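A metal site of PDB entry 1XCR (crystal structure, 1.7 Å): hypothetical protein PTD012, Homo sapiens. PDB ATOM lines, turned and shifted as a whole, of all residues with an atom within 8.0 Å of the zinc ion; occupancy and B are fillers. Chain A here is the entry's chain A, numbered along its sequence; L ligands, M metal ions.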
ATOM      1  N   VAL A  66     -28.052  -2.937   8.569  1.00  0.00           N
ATOM      2  CA  VAL A  66     -27.837  -2.126   9.757  1.00  0.00           C
ATOM      3  C   VAL A  66     -29.165  -1.552  10.305  1.00  0.00           C
ATOM      4  O   VAL A  66     -29.298  -1.432  11.517  1.00  0.00           O
ATOM      5  CB  VAL A  66     -26.779  -1.024   9.513  1.00  0.00           C
ATOM      6  CG1 VAL A  66     -26.695  -0.086  10.716  1.00  0.00           C
ATOM      7  CG2 VAL A  66     -25.395  -1.633   9.248  1.00  0.00           C
ATOM      8  N   ALA A  98     -19.110 -11.209   6.633  1.00  0.00           N
ATOM      9  CA  ALA A  98     -19.163 -10.327   7.804  1.00  0.00           C
ATOM     10  C   ALA A  98     -20.587 -10.111   8.240  1.00  0.00           C
ATOM     11  O   ALA A  98     -21.444  -9.794   7.430  1.00  0.00           O
ATOM     12  CB  ALA A  98     -18.563  -8.978   7.432  1.00  0.00           C
ATOM     13  N   GLY A  99     -20.832 -10.231   9.538  1.00  0.00           N
ATOM     14  CA  GLY A  99     -22.182  -9.989  10.067  1.00  0.00           C
ATOM     15  C   GLY A  99     -22.208  -9.901  11.568  1.00  0.00           C
ATOM     16  O   GLY A  99     -21.159 -10.004  12.221  1.00  0.00           O
ATOM     17  N   ALA A 100     -23.405  -9.690  12.113  1.00  0.00           N
ATOM     18  CA  ALA A 100     -23.613  -9.752  13.558  1.00  0.00           C
ATOM     19  C   ALA A 100     -23.734 -11.230  13.971  1.00  0.00           C
ATOM     20  O   ALA A 100     -24.321 -12.058  13.253  1.00  0.00           O
ATOM     21  CB  ALA A 100     -24.843  -8.932  13.960  1.00  0.00           C
ATOM     22  N   SER A 110     -22.011  -9.953  19.344  1.00  0.00           N
ATOM     23  CA  SER A 110     -20.671 -10.215  18.851  1.00  0.00           C
ATOM     24  C   SER A 110     -20.554  -9.874  17.354  1.00  0.00           C
ATOM     25  O   SER A 110     -21.566  -9.731  16.660  1.00  0.00           O
ATOM     26  CB  SER A 110     -20.296 -11.689  19.067  1.00  0.00           C
ATOM     27  OG  SER A 110     -20.961 -12.559  18.161  1.00  0.00           O
ATOM     28  N   GLU A 111     -19.325  -9.681  16.915  1.00  0.00           N
ATOM     29  CA  GLU A 111     -18.974  -9.582  15.498  1.00  0.00           C
ATOM     30  C   GLU A 111     -18.748 -10.984  14.960  1.00  0.00           C
ATOM     31  O   GLU A 111     -17.952 -11.733  15.543  1.00  0.00           O
ATOM     32  CB  GLU A 111     -17.706  -8.762  15.284  1.00  0.00           C
ATOM     33  CG  GLU A 111     -17.731  -7.349  15.860  1.00  0.00           C
ATOM     34  CD  GLU A 111     -18.771  -6.425  15.253  1.00  0.00           C
ATOM     35  OE1 GLU A 111     -19.198  -6.626  14.094  1.00  0.00           O
ATOM     36  OE2 GLU A 111     -19.188  -5.467  15.941  1.00  0.00           O
ATOM     37  N   PHE A 112     -19.395 -11.323  13.847  1.00  0.00           N
ATOM     38  CA  PHE A 112     -19.351 -12.657  13.278  1.00  0.00           C
ATOM     39  C   PHE A 112     -18.487 -12.722  12.031  1.00  0.00           C
ATOM     40  O   PHE A 112     -18.573 -11.838  11.173  1.00  0.00           O
ATOM     41  CB  PHE A 112     -20.744 -13.170  12.942  1.00  0.00           C
ATOM     42  CG  PHE A 112     -20.884 -14.662  13.054  1.00  0.00           C
ATOM     43  CD1 PHE A 112     -20.658 -15.286  14.284  1.00  0.00           C
ATOM     44  CD2 PHE A 112     -21.282 -15.431  11.974  1.00  0.00           C
ATOM     45  CE1 PHE A 112     -20.800 -16.667  14.418  1.00  0.00           C
ATOM     46  CE2 PHE A 112     -21.422 -16.825  12.126  1.00  0.00           C
ATOM     47  CZ  PHE A 112     -21.182 -17.423  13.352  1.00  0.00           C
ATOM     48  N   MET A 113     -17.667 -13.764  11.941  1.00  0.00           N
ATOM     49  CA  MET A 113     -16.779 -14.012  10.812  1.00  0.00           C
ATOM     50  C   MET A 113     -17.187 -15.358  10.206  1.00  0.00           C
ATOM     51  O   MET A 113     -16.570 -16.385  10.513  1.00  0.00           O
ATOM     52  CB  MET A 113     -15.294 -14.045  11.268  1.00  0.00           C
ATOM     53  CG  MET A 113     -14.630 -12.660  11.441  1.00  0.00           C
ATOM     54  SD  MET A 113     -15.335 -11.635  12.734  1.00  0.00           S
ATOM     55  CE  MET A 113     -14.739 -12.468  14.206  1.00  0.00           C
ATOM     56  N   LEU A 158     -27.913  -8.850  10.248  1.00  0.00           N
ATOM     57  CA  LEU A 158     -27.309  -8.420   9.001  1.00  0.00           C
ATOM     58  C   LEU A 158     -26.141  -9.311   8.652  1.00  0.00           C
ATOM     59  O   LEU A 158     -25.407  -9.752   9.539  1.00  0.00           O
ATOM     60  CB  LEU A 158     -26.863  -6.954   9.072  1.00  0.00           C
ATOM     61  CG  LEU A 158     -25.756  -6.640  10.082  1.00  0.00           C
ATOM     62  CD1 LEU A 158     -24.408  -6.710   9.363  1.00  0.00           C
ATOM     63  CD2 LEU A 158     -25.969  -5.264  10.728  1.00  0.00           C
ATOM     64  N   ASN A 160     -23.198  -9.726   5.240  1.00  0.00           N
ATOM     65  CA  ASN A 160     -22.667  -9.478   3.889  1.00  0.00           C
ATOM     66  C   ASN A 160     -21.754 -10.631   3.568  1.00  0.00           C
ATOM     67  O   ASN A 160     -20.761 -10.852   4.254  1.00  0.00           O
ATOM     68  CB  ASN A 160     -21.963  -8.125   3.833  1.00  0.00           C
ATOM     69  CG  ASN A 160     -22.916  -6.987   4.168  1.00  0.00           C
ATOM     70  OD1 ASN A 160     -22.777  -6.320   5.207  1.00  0.00           O
ATOM     71  ND2 ASN A 160     -23.920  -6.804   3.330  1.00  0.00           N
ATOM     72  N   HIS A 218     -13.410  -2.338  15.261  1.00  0.00           N
ATOM     73  CA  HIS A 218     -14.364  -2.207  16.351  1.00  0.00           C
ATOM     74  C   HIS A 218     -15.042  -3.546  16.657  1.00  0.00           C
ATOM     75  O   HIS A 218     -15.069  -4.447  15.804  1.00  0.00           O
ATOM     76  CB  HIS A 218     -15.401  -1.082  16.093  1.00  0.00           C
ATOM     77  CG  HIS A 218     -16.546  -1.475  15.217  1.00  0.00           C
ATOM     78  ND1 HIS A 218     -16.778  -0.876  14.002  1.00  0.00           N
ATOM     79  CD2 HIS A 218     -17.527  -2.401  15.381  1.00  0.00           C
ATOM     80  CE1 HIS A 218     -17.853  -1.413  13.450  1.00  0.00           C
ATOM     81  NE2 HIS A 218     -18.312  -2.344  14.257  1.00  0.00           N
ATOM     82  N   MET A 220     -18.922  -4.577  18.623  1.00  0.00           N
ATOM     83  CA  MET A 220     -20.143  -4.125  19.318  1.00  0.00           C
ATOM     84  C   MET A 220     -20.176  -4.631  20.757  1.00  0.00           C
ATOM     85  O   MET A 220     -19.767  -5.755  21.018  1.00  0.00           O
ATOM     86  CB  MET A 220     -21.398  -4.673  18.647  1.00  0.00           C
ATOM     87  CG  MET A 220     -21.668  -4.164  17.278  1.00  0.00           C
ATOM     88  SD  MET A 220     -23.195  -4.869  16.615  1.00  0.00           S
ATOM     89  CE  MET A 220     -23.200  -6.573  17.175  1.00  0.00           C
ATOM     90  N   ARG A 264     -24.886  -2.489   1.564  1.00  0.00           N
ATOM     91  CA  ARG A 264     -23.664  -2.134   2.254  1.00  0.00           C
ATOM     92  C   ARG A 264     -22.570  -2.293   1.200  1.00  0.00           C
ATOM     93  O   ARG A 264     -22.309  -3.399   0.726  1.00  0.00           O
ATOM     94  CB  ARG A 264     -23.406  -3.105   3.405  1.00  0.00           C
ATOM     95  CG  ARG A 264     -22.280  -2.706   4.332  1.00  0.00           C
ATOM     96  CD  ARG A 264     -22.718  -1.643   5.275  1.00  0.00           C
ATOM     97  NE  ARG A 264     -21.757  -1.360   6.340  1.00  0.00           N
ATOM     98  CZ  ARG A 264     -21.746  -1.948   7.540  1.00  0.00           C
ATOM     99  NH1 ARG A 264     -22.606  -2.927   7.845  1.00  0.00           N
ATOM    100  NH2 ARG A 264     -20.856  -1.550   8.438  1.00  0.00           N
ATOM    101  N   GLU A 266     -19.255  -1.741   1.386  1.00  0.00           N
ATOM    102  CA  GLU A 266     -17.983  -2.281   1.895  1.00  0.00           C
ATOM    103  C   GLU A 266     -18.190  -2.850   3.277  1.00  0.00           C
ATOM    104  O   GLU A 266     -18.659  -2.148   4.174  1.00  0.00           O
ATOM    105  CB  GLU A 266     -16.909  -1.189   2.019  1.00  0.00           C
ATOM    106  CG  GLU A 266     -16.568  -0.442   0.755  1.00  0.00           C
ATOM    107  CD  GLU A 266     -15.703   0.789   0.994  1.00  0.00           C
ATOM    108  OE1 GLU A 266     -14.868   0.764   1.914  1.00  0.00           O
ATOM    109  OE2 GLU A 266     -15.857   1.789   0.257  1.00  0.00           O
ATOM    110  N   HIS A 267     -17.810  -4.110   3.487  1.00  0.00           N
ATOM    111  CA  HIS A 267     -17.866  -4.682   4.839  1.00  0.00           C
ATOM    112  C   HIS A 267     -16.815  -5.731   4.991  1.00  0.00           C
ATOM    113  O   HIS A 267     -16.835  -6.701   4.236  1.00  0.00           O
ATOM    114  CB  HIS A 267     -19.242  -5.292   5.119  1.00  0.00           C
ATOM    115  CG  HIS A 267     -19.580  -5.415   6.573  1.00  0.00           C
ATOM    116  ND1 HIS A 267     -20.749  -6.011   6.994  1.00  0.00           N
ATOM    117  CD2 HIS A 267     -18.910  -5.050   7.693  1.00  0.00           C
ATOM    118  CE1 HIS A 267     -20.797  -5.980   8.308  1.00  0.00           C
ATOM    119  NE2 HIS A 267     -19.688  -5.405   8.768  1.00  0.00           N
ATOM    120  N   THR A 268     -15.937  -5.566   5.983  1.00  0.00           N
ATOM    121  CA  THR A 268     -14.830  -6.504   6.193  1.00  0.00           C
ATOM    122  C   THR A 268     -14.700  -6.863   7.675  1.00  0.00           C
ATOM    123  O   THR A 268     -14.550  -5.987   8.512  1.00  0.00           O
ATOM    124  CB  THR A 268     -13.485  -5.922   5.731  1.00  0.00           C
ATOM    125  OG1 THR A 268     -13.576  -5.498   4.367  1.00  0.00           O
ATOM    126  CG2 THR A 268     -12.365  -6.947   5.862  1.00  0.00           C
ATOM    127  N   HIS A 269     -14.759  -8.163   7.965  1.00  0.00           N
ATOM    128  CA  HIS A 269     -14.487  -8.667   9.306  1.00  0.00           C
ATOM    129  C   HIS A 269     -13.231  -9.536   9.275  1.00  0.00           C
ATOM    130  O   HIS A 269     -12.845 -10.013   8.223  1.00  0.00           O
ATOM    131  CB  HIS A 269     -15.670  -9.456   9.840  1.00  0.00           C
ATOM    132  CG  HIS A 269     -16.775  -8.597  10.403  1.00  0.00           C
ATOM    133  ND1 HIS A 269     -17.771  -9.123  11.190  1.00  0.00           N
ATOM    134  CD2 HIS A 269     -17.038  -7.278  10.296  1.00  0.00           C
ATOM    135  CE1 HIS A 269     -18.597  -8.153  11.552  1.00  0.00           C
ATOM    136  NE2 HIS A 269     -18.178  -7.019  11.019  1.00  0.00           N
ATOM    137  N   PHE A 270     -12.590  -9.725  10.422  1.00  0.00           N
ATOM    138  CA  PHE A 270     -11.358 -10.523  10.424  1.00  0.00           C
ATOM    139  C   PHE A 270     -11.196 -11.326  11.715  1.00  0.00           C
ATOM    140  O   PHE A 270     -11.870 -11.077  12.728  1.00  0.00           O
ATOM    141  CB  PHE A 270     -10.146  -9.613  10.204  1.00  0.00           C
ATOM    142  CG  PHE A 270      -9.982  -8.549  11.255  1.00  0.00           C
ATOM    143  CD1 PHE A 270      -9.250  -8.806  12.406  1.00  0.00           C
ATOM    144  CD2 PHE A 270     -10.591  -7.313  11.094  1.00  0.00           C
ATOM    145  CE1 PHE A 270      -9.127  -7.827  13.395  1.00  0.00           C
ATOM    146  CE2 PHE A 270     -10.464  -6.340  12.063  1.00  0.00           C
ATOM    147  CZ  PHE A 270      -9.733  -6.599  13.223  1.00  0.00           C
ATOM    148  N   GLY A 278     -12.686  -8.737  14.591  1.00  0.00           N
ATOM    149  CA  GLY A 278     -13.754  -7.744  14.601  1.00  0.00           C
ATOM    150  C   GLY A 278     -13.959  -7.131  13.237  1.00  0.00           C
ATOM    151  O   GLY A 278     -13.691  -7.765  12.216  1.00  0.00           O
ATOM    152  N   HIS A 279     -14.418  -5.883  13.254  1.00  0.00           N
ATOM    153  CA  HIS A 279     -14.806  -5.117  12.082  1.00  0.00           C
ATOM    154  C   HIS A 279     -13.673  -4.179  11.697  1.00  0.00           C
ATOM    155  O   HIS A 279     -13.254  -3.354  12.504  1.00  0.00           O
ATOM    156  CB  HIS A 279     -16.092  -4.322  12.413  1.00  0.00           C
ATOM    157  CG  HIS A 279     -16.534  -3.366  11.337  1.00  0.00           C
ATOM    158  ND1 HIS A 279     -17.747  -3.502  10.682  1.00  0.00           N
ATOM    159  CD2 HIS A 279     -15.971  -2.240  10.844  1.00  0.00           C
ATOM    160  CE1 HIS A 279     -17.881  -2.516   9.821  1.00  0.00           C
ATOM    161  NE2 HIS A 279     -16.819  -1.737   9.900  1.00  0.00           N
ATOM    162  N   TYR A 280     -13.185  -4.327  10.465  1.00  0.00           N
ATOM    163  CA  TYR A 280     -12.057  -3.533   9.938  1.00  0.00           C
ATOM    164  C   TYR A 280     -12.438  -2.114   9.495  1.00  0.00           C
ATOM    165  O   TYR A 280     -13.378  -1.937   8.732  1.00  0.00           O
ATOM    166  CB  TYR A 280     -11.435  -4.307   8.751  1.00  0.00           C
ATOM    167  CG  TYR A 280     -10.415  -3.572   7.906  1.00  0.00           C
ATOM    168  CD1 TYR A 280      -9.073  -3.507   8.290  1.00  0.00           C
ATOM    169  CD2 TYR A 280     -10.765  -2.998   6.687  1.00  0.00           C
ATOM    170  CE1 TYR A 280      -8.128  -2.869   7.501  1.00  0.00           C
ATOM    171  CE2 TYR A 280      -9.841  -2.396   5.890  1.00  0.00           C
ATOM    172  CZ  TYR A 280      -8.515  -2.318   6.295  1.00  0.00           C
ATOM    173  OH  TYR A 280      -7.593  -1.707   5.499  1.00  0.00           O
ATOM    174  N   HIS A 281     -11.690  -1.110   9.974  1.00  0.00           N
ATOM    175  CA  HIS A 281     -11.853   0.280   9.522  1.00  0.00           C
ATOM    176  C   HIS A 281     -10.760   0.702   8.536  1.00  0.00           C
ATOM    177  O   HIS A 281     -11.068   1.082   7.403  1.00  0.00           O
ATOM    178  CB  HIS A 281     -11.944   1.254  10.709  1.00  0.00           C
ATOM    179  CG  HIS A 281     -13.255   1.188  11.423  1.00  0.00           C
ATOM    180  ND1 HIS A 281     -14.291   2.053  11.143  1.00  0.00           N
ATOM    181  CD2 HIS A 281     -13.710   0.330  12.358  1.00  0.00           C
ATOM    182  CE1 HIS A 281     -15.335   1.722  11.885  1.00  0.00           C
ATOM    183  NE2 HIS A 281     -15.014   0.686  12.628  1.00  0.00           N
ATOM    184  N   GLY A 314     -24.674   4.314  10.520  1.00  0.00           N
ATOM    185  CA  GLY A 314     -23.943   3.200  11.084  1.00  0.00           C
ATOM    186  C   GLY A 314     -23.304   2.271  10.082  1.00  0.00           C
ATOM    187  O   GLY A 314     -23.069   1.106  10.402  1.00  0.00           O
ATOM    188  N   ARG A 315     -22.986   2.767   8.877  1.00  0.00           N
ATOM    189  CA  ARG A 315     -22.502   1.912   7.796  1.00  0.00           C
ATOM    190  C   ARG A 315     -20.988   1.841   7.643  1.00  0.00           C
ATOM    191  O   ARG A 315     -20.494   1.030   6.858  1.00  0.00           O
ATOM    192  CB  ARG A 315     -23.112   2.315   6.450  1.00  0.00           C
ATOM    193  CG  ARG A 315     -24.618   2.309   6.466  1.00  0.00           C
ATOM    194  CD  ARG A 315     -25.245   1.477   5.355  1.00  0.00           C
ATOM    195  NE  ARG A 315     -26.701   1.477   5.529  1.00  0.00           N
ATOM    196  CZ  ARG A 315     -27.569   0.940   4.676  1.00  0.00           C
ATOM    197  NH1 ARG A 315     -27.164   0.356   3.552  1.00  0.00           N
ATOM    198  NH2 ARG A 315     -28.869   1.009   4.958  1.00  0.00           N
ATOM    199  N   ASP A 316     -20.245   2.656   8.391  1.00  0.00           N
ATOM    200  CA  ASP A 316     -18.783   2.538   8.408  1.00  0.00           C
ATOM    201  C   ASP A 316     -18.358   1.178   8.948  1.00  0.00           C
ATOM    202  O   ASP A 316     -19.029   0.606   9.823  1.00  0.00           O
ATOM    203  CB  ASP A 316     -18.140   3.636   9.247  1.00  0.00           C
ATOM    204  CG  ASP A 316     -18.359   5.021   8.676  1.00  0.00           C
ATOM    205  OD1 ASP A 316     -19.042   5.127   7.621  1.00  0.00           O
ATOM    206  OD2 ASP A 316     -17.861   6.002   9.275  1.00  0.00           O
ATOM    207  OXT ASP A 316     -17.327   0.645   8.508  1.00  0.00           O
HETATM  208  C1  LIG L   1     -21.674  -5.781  12.039  1.00  0.00           C
HETATM  209  O1  LIG L   1     -22.665  -5.708  12.807  1.00  0.00           O
HETATM  210  O2  LIG L   1     -20.822  -4.894  11.827  1.00  0.00           O
HETATM  211  C2  LIG L   1     -21.492  -7.042  11.301  1.00  0.00           C
HETATM  212 ZN    ZN M   1     -19.095  -5.188  10.691  1.00  0.00          ZN
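A ring nitrogen (ND1) of His 267 lies within hydrogen-bond range of the side-chain amide oxygen (OD1) of Asn 160, 2.7 Å away.
OE1 of Glu 111 lies close to NE2 of His 269, at 3.3 Å.
ND1 of His 269 is in hydrogen-bond range of O of Phe 112.
O of His 279 lies within hydrogen-bond range of N of His 218 (2.9 Å).
The chain-end carboxylate (OXT) of Asp 316 sits at hydrogen-bond distance from a ring nitrogen (NE2) of His 279.
OE2 of Glu 111 sits at hydrogen-bond distance from N of Met 220.
A ring nitrogen (NE2) of His 267 binds the zinc ion (2.0 Å).
A ring nitrogen (NE2) of His 269 is bound to the zinc ion.
O2 of the ligand binds the zinc ion (2.1 Å).
ND1 of His 279 binds the zinc ion (2.2 Å).
The zinc ion has four donor atoms within binding distance.
Merely in contact with the zinc ion: Glu 111.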
